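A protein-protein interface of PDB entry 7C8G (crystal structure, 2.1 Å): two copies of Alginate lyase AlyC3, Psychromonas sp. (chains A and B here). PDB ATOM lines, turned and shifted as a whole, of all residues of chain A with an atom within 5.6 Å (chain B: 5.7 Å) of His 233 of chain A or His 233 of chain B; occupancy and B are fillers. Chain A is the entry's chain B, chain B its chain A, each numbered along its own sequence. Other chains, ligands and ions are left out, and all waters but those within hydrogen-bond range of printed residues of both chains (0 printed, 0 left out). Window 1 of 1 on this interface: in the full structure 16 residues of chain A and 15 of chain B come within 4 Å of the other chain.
Of chain B, only Arg 232 and His 233 come within 4 Å of His 233 of chain A. Of the printed residues of chain A, His 233 of chain B touches Arg 232 (3.4 Å) and His 233 (3.4 Å). Of the printed residues of chain B, Asp 89 of chain A touches Arg 232. Of the printed residues of chain B, Arg 232 of chain A touches Asp 89 (2.9 Å), Arg 232 (2.8 Å) and His 233 (3.4 Å). Of the printed residues of chain A, Arg 232 of chain B touches Asp 89 (3.1 Å), Arg 232 (2.8 Å) and His 233 (3.6 Å). Of the printed residues of chain A, Asp 89 of chain B touches Arg 232. Of the printed residues of chain A, Ala 166 of chain B touches Leu 130. Tyr 230 of chain A touches none of the printed residues of chain B. Gly 129 of chain A touches none of the printed residues of chain B.
Printed residues of chain B that touch a printed residue of chain A: Asp 89, Leu 130, Ala 166, Arg 232 and His 233. Hydrophobic or aromatic side chains of chain B that line the printed part of chain A: Leu 130 and His 233. Among the printed residues, 8 pairs touch across the chains. Among the printed residues, Asp or Glu carboxylates within 4 Å of a Lys or Arg side-chain nitrogen of the other chain: Asp 89 of chain A with Arg 232 of chain B and Arg 232 of chain A with Asp 89 of chain B.
O of Arg 232 of chain B lies within hydrogen-bond range of NH2 of Arg 232 of chain A. The side-chain carboxylate (OD2) of Asp 89 of chain A is in salt-bridge range of the guanidinium group (NE) of Arg 232 of chain B (3.1 Å). The side-chain carboxylate (OD2) of Asp 89 of chain B is in salt-bridge range of the guanidinium group (NE) of Arg 232 of chain A, 2.9 Å away.
NH1 of Arg 232 of chain A is in salt-bridge range of OD1 of Asp 229 of chain A, 3.4 Å away. The side-chain carboxylate (OD1) of Asp 229 of chain B is in salt-bridge range of the guanidinium group (NH1) of Arg 232 of chain B (3.4 Å).
Among the printed residues, merely in contact across the chains: His 233 of chain A with His 233 of chain B (3.4 Å), Arg 232 of chain A with His 233 of chain B (3.4 Å), Ala 166 of chain A with Leu 130 of chain B (3.5 Å), Leu 130 of chain A with Ala 166 of chain B (3.6 Å) and His 233 of chain A with Arg 232 of chain B (3.6 Å).
Asp 89 of chain A touches Arg 232 of chain B, and with the chains exchanged Arg 232 of chain A touches Asp 89 of chain B. Arg 232 of chain A touches its own counterpart, Arg 232 of chain B. Arg 232 of chain A touches His 233 of chain B, and with the chains exchanged His 233 of chain A touches Arg 232 of chain B. His 233 of chain A touches its own counterpart, His 233 of chain B.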
ATOM      1  N   ASP A  89     -14.919 -10.099 -14.110  1.00  0.00           N
ATOM      2  CA  ASP A  89     -13.505 -10.091 -14.449  1.00  0.00           C
ATOM      3  C   ASP A  89     -13.197  -9.468 -15.808  1.00  0.00           C
ATOM      4  O   ASP A  89     -12.028  -9.445 -16.212  1.00  0.00           O
ATOM      5  CB  ASP A  89     -12.948 -11.528 -14.377  1.00  0.00           C
ATOM      6  CG  ASP A  89     -13.665 -12.492 -15.316  1.00  0.00           C
ATOM      7  OD1 ASP A  89     -14.873 -12.315 -15.578  1.00  0.00           O
ATOM      8  OD2 ASP A  89     -13.009 -13.429 -15.815  1.00  0.00           O
ATOM      9  N   GLY A 129     -23.217 -18.401  -9.314  1.00  0.00           N
ATOM     10  CA  GLY A 129     -22.456 -19.617  -9.446  1.00  0.00           C
ATOM     11  C   GLY A 129     -21.655 -19.571 -10.733  1.00  0.00           C
ATOM     12  O   GLY A 129     -21.433 -18.501 -11.297  1.00  0.00           O
ATOM     13  N   LEU A 130     -21.244 -20.759 -11.188  1.00  0.00           N
ATOM     14  CA  LEU A 130     -20.486 -20.853 -12.428  1.00  0.00           C
ATOM     15  C   LEU A 130     -21.312 -20.433 -13.634  1.00  0.00           C
ATOM     16  O   LEU A 130     -20.746 -19.990 -14.636  1.00  0.00           O
ATOM     17  CB  LEU A 130     -19.978 -22.281 -12.634  1.00  0.00           C
ATOM     18  CG  LEU A 130     -18.905 -22.728 -11.650  1.00  0.00           C
ATOM     19  CD1 LEU A 130     -18.475 -24.198 -11.932  1.00  0.00           C
ATOM     20  CD2 LEU A 130     -17.736 -21.763 -11.739  1.00  0.00           C
ATOM     21  N   VAL A 138     -21.552 -20.407  -4.387  1.00  0.00           N
ATOM     22  CA  VAL A 138     -20.841 -20.167  -3.143  1.00  0.00           C
ATOM     23  C   VAL A 138     -21.800 -19.431  -2.212  1.00  0.00           C
ATOM     24  O   VAL A 138     -22.273 -18.341  -2.576  1.00  0.00           O
ATOM     25  CB  VAL A 138     -19.563 -19.352  -3.376  1.00  0.00           C
ATOM     26  CG1 VAL A 138     -18.889 -19.018  -2.050  1.00  0.00           C
ATOM     27  CG2 VAL A 138     -18.605 -20.140  -4.314  1.00  0.00           C
ATOM     28  N   ALA A 166     -12.887 -17.368  -2.780  1.00  0.00           N
ATOM     29  CA  ALA A 166     -14.035 -18.029  -3.390  1.00  0.00           C
ATOM     30  C   ALA A 166     -14.325 -19.379  -2.745  1.00  0.00           C
ATOM     31  O   ALA A 166     -14.781 -20.312  -3.411  1.00  0.00           O
ATOM     32  CB  ALA A 166     -13.820 -18.180  -4.897  1.00  0.00           C
ATOM     33  N   ASP A 229      -9.806 -10.673  -8.382  1.00  0.00           N
ATOM     34  CA  ASP A 229      -9.334 -11.713  -9.287  1.00  0.00           C
ATOM     35  C   ASP A 229      -9.794 -13.089  -8.824  1.00  0.00           C
ATOM     36  O   ASP A 229     -10.171 -13.935  -9.642  1.00  0.00           O
ATOM     37  CB  ASP A 229      -7.809 -11.642  -9.366  1.00  0.00           C
ATOM     38  CG  ASP A 229      -7.227 -12.472 -10.499  1.00  0.00           C
ATOM     39  OD1 ASP A 229      -7.967 -12.951 -11.386  1.00  0.00           O
ATOM     40  OD2 ASP A 229      -6.002 -12.630 -10.505  1.00  0.00           O
ATOM     41  N   TYR A 230      -9.807 -13.312  -7.507  1.00  0.00           N
ATOM     42  CA  TYR A 230     -10.159 -14.614  -6.942  1.00  0.00           C
ATOM     43  C   TYR A 230     -11.588 -15.026  -7.248  1.00  0.00           C
ATOM     44  O   TYR A 230     -11.915 -16.211  -7.133  1.00  0.00           O
ATOM     45  CB  TYR A 230      -9.968 -14.600  -5.425  1.00  0.00           C
ATOM     46  CG  TYR A 230     -10.723 -13.483  -4.713  1.00  0.00           C
ATOM     47  CD1 TYR A 230     -12.021 -13.677  -4.254  1.00  0.00           C
ATOM     48  CD2 TYR A 230     -10.125 -12.244  -4.482  1.00  0.00           C
ATOM     49  CE1 TYR A 230     -12.705 -12.683  -3.586  1.00  0.00           C
ATOM     50  CE2 TYR A 230     -10.810 -11.222  -3.813  1.00  0.00           C
ATOM     51  CZ  TYR A 230     -12.097 -11.456  -3.372  1.00  0.00           C
ATOM     52  OH  TYR A 230     -12.784 -10.468  -2.712  1.00  0.00           O
ATOM     53  N   TRP A 231     -12.442 -14.069  -7.601  1.00  0.00           N
ATOM     54  CA  TRP A 231     -13.862 -14.263  -7.844  1.00  0.00           C
ATOM     55  C   TRP A 231     -14.179 -14.479  -9.323  1.00  0.00           C
ATOM     56  O   TRP A 231     -15.343 -14.721  -9.665  1.00  0.00           O
ATOM     57  CB  TRP A 231     -14.619 -13.019  -7.312  1.00  0.00           C
ATOM     58  CG  TRP A 231     -16.065 -13.177  -6.948  1.00  0.00           C
ATOM     59  CD1 TRP A 231     -17.146 -12.743  -7.675  1.00  0.00           C
ATOM     60  CD2 TRP A 231     -16.599 -13.749  -5.745  1.00  0.00           C
ATOM     61  NE1 TRP A 231     -18.320 -13.035  -7.007  1.00  0.00           N
ATOM     62  CE2 TRP A 231     -18.012 -13.651  -5.823  1.00  0.00           C
ATOM     63  CE3 TRP A 231     -16.024 -14.347  -4.616  1.00  0.00           C
ATOM     64  CZ2 TRP A 231     -18.856 -14.124  -4.814  1.00  0.00           C
ATOM     65  CZ3 TRP A 231     -16.862 -14.827  -3.617  1.00  0.00           C
ATOM     66  CH2 TRP A 231     -18.268 -14.709  -3.725  1.00  0.00           C
ATOM     67  N   ARG A 232     -13.165 -14.435 -10.195  1.00  0.00           N
ATOM     68  CA  ARG A 232     -13.397 -14.254 -11.630  1.00  0.00           C
ATOM     69  C   ARG A 232     -14.369 -15.267 -12.223  1.00  0.00           C
ATOM     70  O   ARG A 232     -15.072 -14.960 -13.192  1.00  0.00           O
ATOM     71  CB  ARG A 232     -12.064 -14.313 -12.372  1.00  0.00           C
ATOM     72  CG  ARG A 232     -11.272 -15.602 -12.158  1.00  0.00           C
ATOM     73  CD  ARG A 232      -9.867 -15.439 -12.752  1.00  0.00           C
ATOM     74  NE  ARG A 232      -9.027 -16.624 -12.601  1.00  0.00           N
ATOM     75  CZ  ARG A 232      -8.360 -16.928 -11.489  1.00  0.00           C
ATOM     76  NH1 ARG A 232      -8.454 -16.136 -10.418  1.00  0.00           N
ATOM     77  NH2 ARG A 232      -7.594 -18.024 -11.444  1.00  0.00           N
ATOM     78  N   HIS A 233     -14.447 -16.460 -11.653  1.00  0.00           N
ATOM     79  CA  HIS A 233     -15.294 -17.502 -12.215  1.00  0.00           C
ATOM     80  C   HIS A 233     -16.761 -17.382 -11.837  1.00  0.00           C
ATOM     81  O   HIS A 233     -17.578 -18.113 -12.398  1.00  0.00           O
ATOM     82  CB  HIS A 233     -14.784 -18.883 -11.778  1.00  0.00           C
ATOM     83  CG  HIS A 233     -14.659 -19.054 -10.295  1.00  0.00           C
ATOM     84  ND1 HIS A 233     -13.834 -18.268  -9.518  1.00  0.00           N
ATOM     85  CD2 HIS A 233     -15.227 -19.950  -9.452  1.00  0.00           C
ATOM     86  CE1 HIS A 233     -13.904 -18.669  -8.259  1.00  0.00           C
ATOM     87  NE2 HIS A 233     -14.747 -19.684  -8.191  1.00  0.00           N
ATOM     88  N   LEU A 234     -17.121 -16.507 -10.906  1.00  0.00           N
ATOM     89  CA  LEU A 234     -18.450 -16.517 -10.308  1.00  0.00           C
ATOM     90  C   LEU A 234     -19.321 -15.434 -10.950  1.00  0.00           C
ATOM     91  O   LEU A 234     -19.071 -14.236 -10.776  1.00  0.00           O
ATOM     92  CB  LEU A 234     -18.344 -16.327  -8.794  1.00  0.00           C
ATOM     93  CG  LEU A 234     -17.604 -17.460  -8.063  1.00  0.00           C
ATOM     94  CD1 LEU A 234     -17.484 -17.175  -6.556  1.00  0.00           C
ATOM     95  CD2 LEU A 234     -18.330 -18.765  -8.307  1.00  0.00           C
ATOM     96  N   LEU A 235     -20.340 -15.857 -11.687  1.00  0.00           N
ATOM     97  CA  LEU A 235     -21.358 -14.922 -12.149  1.00  0.00           C
ATOM     98  C   LEU A 235     -22.024 -14.283 -10.938  1.00  0.00           C
ATOM     99  O   LEU A 235     -22.431 -14.980 -10.005  1.00  0.00           O
ATOM    100  CB  LEU A 235     -22.399 -15.640 -13.008  1.00  0.00           C
ATOM    101  CG  LEU A 235     -22.301 -15.603 -14.529  1.00  0.00           C
ATOM    102  CD1 LEU A 235     -20.871 -15.406 -15.004  1.00  0.00           C
ATOM    103  CD2 LEU A 235     -22.919 -16.863 -15.137  1.00  0.00           C
ATOM    104  N   ASP B  89      -5.121 -19.000 -17.396  1.00  0.00           N
ATOM    105  CA  ASP B  89      -5.875 -17.918 -18.007  1.00  0.00           C
ATOM    106  C   ASP B  89      -5.044 -16.672 -18.295  1.00  0.00           C
ATOM    107  O   ASP B  89      -5.598 -15.675 -18.769  1.00  0.00           O
ATOM    108  CB  ASP B  89      -7.094 -17.565 -17.140  1.00  0.00           C
ATOM    109  CG  ASP B  89      -6.736 -17.187 -15.703  1.00  0.00           C
ATOM    110  OD1 ASP B  89      -5.682 -17.608 -15.173  1.00  0.00           O
ATOM    111  OD2 ASP B  89      -7.551 -16.471 -15.080  1.00  0.00           O
ATOM    112  N   GLY B 129      -6.956 -27.200  -7.957  1.00  0.00           N
ATOM    113  CA  GLY B 129      -8.110 -26.594  -7.336  1.00  0.00           C
ATOM    114  C   GLY B 129      -7.993 -25.082  -7.399  1.00  0.00           C
ATOM    115  O   GLY B 129      -7.290 -24.534  -8.248  1.00  0.00           O
ATOM    116  N   LEU B 130      -8.708 -24.422  -6.481  1.00  0.00           N
ATOM    117  CA  LEU B 130      -8.655 -22.966  -6.384  1.00  0.00           C
ATOM    118  C   LEU B 130      -7.267 -22.468  -5.992  1.00  0.00           C
ATOM    119  O   LEU B 130      -6.898 -21.340  -6.332  1.00  0.00           O
ATOM    120  CB  LEU B 130      -9.670 -22.476  -5.351  1.00  0.00           C
ATOM    121  CG  LEU B 130     -10.960 -21.743  -5.690  1.00  0.00           C
ATOM    122  CD1 LEU B 130     -11.445 -21.912  -7.130  1.00  0.00           C
ATOM    123  CD2 LEU B 130     -12.058 -22.132  -4.680  1.00  0.00           C
ATOM    124  N   ASP B 131      -6.498 -23.272  -5.257  1.00  0.00           N
ATOM    125  CA  ASP B 131      -5.245 -22.824  -4.664  1.00  0.00           C
ATOM    126  C   ASP B 131      -4.253 -23.988  -4.648  1.00  0.00           C
ATOM    127  O   ASP B 131      -4.565 -25.104  -5.073  1.00  0.00           O
ATOM    128  CB  ASP B 131      -5.478 -22.270  -3.247  1.00  0.00           C
ATOM    129  CG  ASP B 131      -6.262 -23.232  -2.363  1.00  0.00           C
ATOM    130  OD1 ASP B 131      -6.120 -24.470  -2.513  1.00  0.00           O
ATOM    131  OD2 ASP B 131      -7.044 -22.763  -1.518  1.00  0.00           O
ATOM    132  N   VAL B 138     -11.694 -30.124  -8.601  1.00  0.00           N
ATOM    133  CA  VAL B 138     -12.659 -30.735  -9.511  1.00  0.00           C
ATOM    134  C   VAL B 138     -12.116 -32.110  -9.889  1.00  0.00           C
ATOM    135  O   VAL B 138     -11.000 -32.185 -10.423  1.00  0.00           O
ATOM    136  CB  VAL B 138     -12.889 -29.872 -10.757  1.00  0.00           C
ATOM    137  CG1 VAL B 138     -13.794 -30.591 -11.755  1.00  0.00           C
ATOM    138  CG2 VAL B 138     -13.491 -28.510 -10.355  1.00  0.00           C
ATOM    139  N   ALA B 166     -16.345 -26.658 -15.867  1.00  0.00           N
ATOM    140  CA  ALA B 166     -15.674 -26.791 -14.582  1.00  0.00           C
ATOM    141  C   ALA B 166     -16.579 -27.427 -13.536  1.00  0.00           C
ATOM    142  O   ALA B 166     -16.461 -27.138 -12.344  1.00  0.00           O
ATOM    143  CB  ALA B 166     -15.151 -25.436 -14.108  1.00  0.00           C
ATOM    144  N   ASP B 229     -11.629 -20.672 -21.159  1.00  0.00           N
ATOM    145  CA  ASP B 229     -12.076 -19.599 -20.288  1.00  0.00           C
ATOM    146  C   ASP B 229     -12.840 -20.159 -19.093  1.00  0.00           C
ATOM    147  O   ASP B 229     -12.668 -19.692 -17.961  1.00  0.00           O
ATOM    148  CB  ASP B 229     -12.935 -18.639 -21.116  1.00  0.00           C
ATOM    149  CG  ASP B 229     -13.358 -17.416 -20.353  1.00  0.00           C
ATOM    150  OD1 ASP B 229     -12.654 -16.986 -19.423  1.00  0.00           O
ATOM    151  OD2 ASP B 229     -14.411 -16.871 -20.712  1.00  0.00           O
ATOM    152  N   TYR B 230     -13.635 -21.212 -19.324  1.00  0.00           N
ATOM    153  CA  TYR B 230     -14.460 -21.817 -18.282  1.00  0.00           C
ATOM    154  C   TYR B 230     -13.638 -22.406 -17.142  1.00  0.00           C
ATOM    155  O   TYR B 230     -14.188 -22.711 -16.075  1.00  0.00           O
ATOM    156  CB  TYR B 230     -15.333 -22.911 -18.898  1.00  0.00           C
ATOM    157  CG  TYR B 230     -14.541 -24.017 -19.598  1.00  0.00           C
ATOM    158  CD1 TYR B 230     -14.032 -25.112 -18.891  1.00  0.00           C
ATOM    159  CD2 TYR B 230     -14.316 -23.970 -20.966  1.00  0.00           C
ATOM    160  CE1 TYR B 230     -13.309 -26.130 -19.553  1.00  0.00           C
ATOM    161  CE2 TYR B 230     -13.592 -24.978 -21.633  1.00  0.00           C
ATOM    162  CZ  TYR B 230     -13.098 -26.046 -20.929  1.00  0.00           C
ATOM    163  OH  TYR B 230     -12.400 -27.021 -21.616  1.00  0.00           O
ATOM    164  N   TRP B 231     -12.341 -22.586 -17.357  1.00  0.00           N
ATOM    165  CA  TRP B 231     -11.438 -23.247 -16.425  1.00  0.00           C
ATOM    166  C   TRP B 231     -10.566 -22.244 -15.687  1.00  0.00           C
ATOM    167  O   TRP B 231      -9.651 -22.648 -14.963  1.00  0.00           O
ATOM    168  CB  TRP B 231     -10.567 -24.230 -17.215  1.00  0.00           C
ATOM    169  CG  TRP B 231      -9.882 -25.364 -16.496  1.00  0.00           C
ATOM    170  CD1 TRP B 231      -8.572 -25.422 -16.139  1.00  0.00           C
ATOM    171  CD2 TRP B 231     -10.456 -26.626 -16.124  1.00  0.00           C
ATOM    172  NE1 TRP B 231      -8.295 -26.630 -15.544  1.00  0.00           N
ATOM    173  CE2 TRP B 231      -9.435 -27.389 -15.528  1.00  0.00           C
ATOM    174  CE3 TRP B 231     -11.741 -27.177 -16.225  1.00  0.00           C
ATOM    175  CZ2 TRP B 231      -9.650 -28.687 -15.037  1.00  0.00           C
ATOM    176  CZ3 TRP B 231     -11.960 -28.459 -15.728  1.00  0.00           C
ATOM    177  CH2 TRP B 231     -10.914 -29.201 -15.142  1.00  0.00           C
ATOM    178  N   ARG B 232     -10.831 -20.943 -15.868  1.00  0.00           N
ATOM    179  CA  ARG B 232      -9.849 -19.914 -15.538  1.00  0.00           C
ATOM    180  C   ARG B 232      -9.469 -19.905 -14.064  1.00  0.00           C
ATOM    181  O   ARG B 232      -8.339 -19.533 -13.725  1.00  0.00           O
ATOM    182  CB  ARG B 232     -10.375 -18.536 -15.954  1.00  0.00           C
ATOM    183  CG  ARG B 232     -11.694 -18.111 -15.305  1.00  0.00           C
ATOM    184  CD  ARG B 232     -12.222 -16.847 -16.025  1.00  0.00           C
ATOM    185  NE  ARG B 232     -13.554 -16.434 -15.604  1.00  0.00           N
ATOM    186  CZ  ARG B 232     -14.680 -16.978 -16.049  1.00  0.00           C
ATOM    187  NH1 ARG B 232     -14.637 -17.987 -16.909  1.00  0.00           N
ATOM    188  NH2 ARG B 232     -15.853 -16.516 -15.626  1.00  0.00           N
ATOM    189  N   HIS B 233     -10.378 -20.315 -13.179  1.00  0.00           N
ATOM    190  CA  HIS B 233     -10.141 -20.266 -11.737  1.00  0.00           C
ATOM    191  C   HIS B 233      -9.340 -21.445 -11.194  1.00  0.00           C
ATOM    192  O   HIS B 233      -8.963 -21.427 -10.017  1.00  0.00           O
ATOM    193  CB  HIS B 233     -11.467 -20.230 -10.993  1.00  0.00           C
ATOM    194  CG  HIS B 233     -12.396 -21.340 -11.374  1.00  0.00           C
ATOM    195  ND1 HIS B 233     -12.804 -21.556 -12.674  1.00  0.00           N
ATOM    196  CD2 HIS B 233     -13.007 -22.288 -10.626  1.00  0.00           C
ATOM    197  CE1 HIS B 233     -13.619 -22.595 -12.708  1.00  0.00           C
ATOM    198  NE2 HIS B 233     -13.765 -23.053 -11.476  1.00  0.00           N
ATOM    199  N   LEU B 234      -9.099 -22.474 -11.989  1.00  0.00           N
ATOM    200  CA  LEU B 234      -8.509 -23.711 -11.492  1.00  0.00           C
ATOM    201  C   LEU B 234      -7.009 -23.740 -11.792  1.00  0.00           C
ATOM    202  O   LEU B 234      -6.606 -23.755 -12.961  1.00  0.00           O
ATOM    203  CB  LEU B 234      -9.225 -24.911 -12.114  1.00  0.00           C
ATOM    204  CG  LEU B 234     -10.687 -25.052 -11.670  1.00  0.00           C
ATOM    205  CD1 LEU B 234     -11.394 -26.165 -12.430  1.00  0.00           C
ATOM    206  CD2 LEU B 234     -10.737 -25.322 -10.191  1.00  0.00           C
ATOM    207  N   LEU B 235      -6.187 -23.732 -10.740  1.00  0.00           N
ATOM    208  CA  LEU B 235      -4.766 -24.001 -10.925  1.00  0.00           C
ATOM    209  C   LEU B 235      -4.589 -25.423 -11.441  1.00  0.00           C
ATOM    210  O   LEU B 235      -5.244 -26.352 -10.969  1.00  0.00           O
ATOM    211  CB  LEU B 235      -3.991 -23.810  -9.620  1.00  0.00           C
ATOM    212  CG  LEU B 235      -4.118 -22.427  -8.967  1.00  0.00           C
ATOM    213  CD1 LEU B 235      -3.230 -22.339  -7.729  1.00  0.00           C
ATOM    214  CD2 LEU B 235      -3.802 -21.298  -9.972  1.00  0.00           C
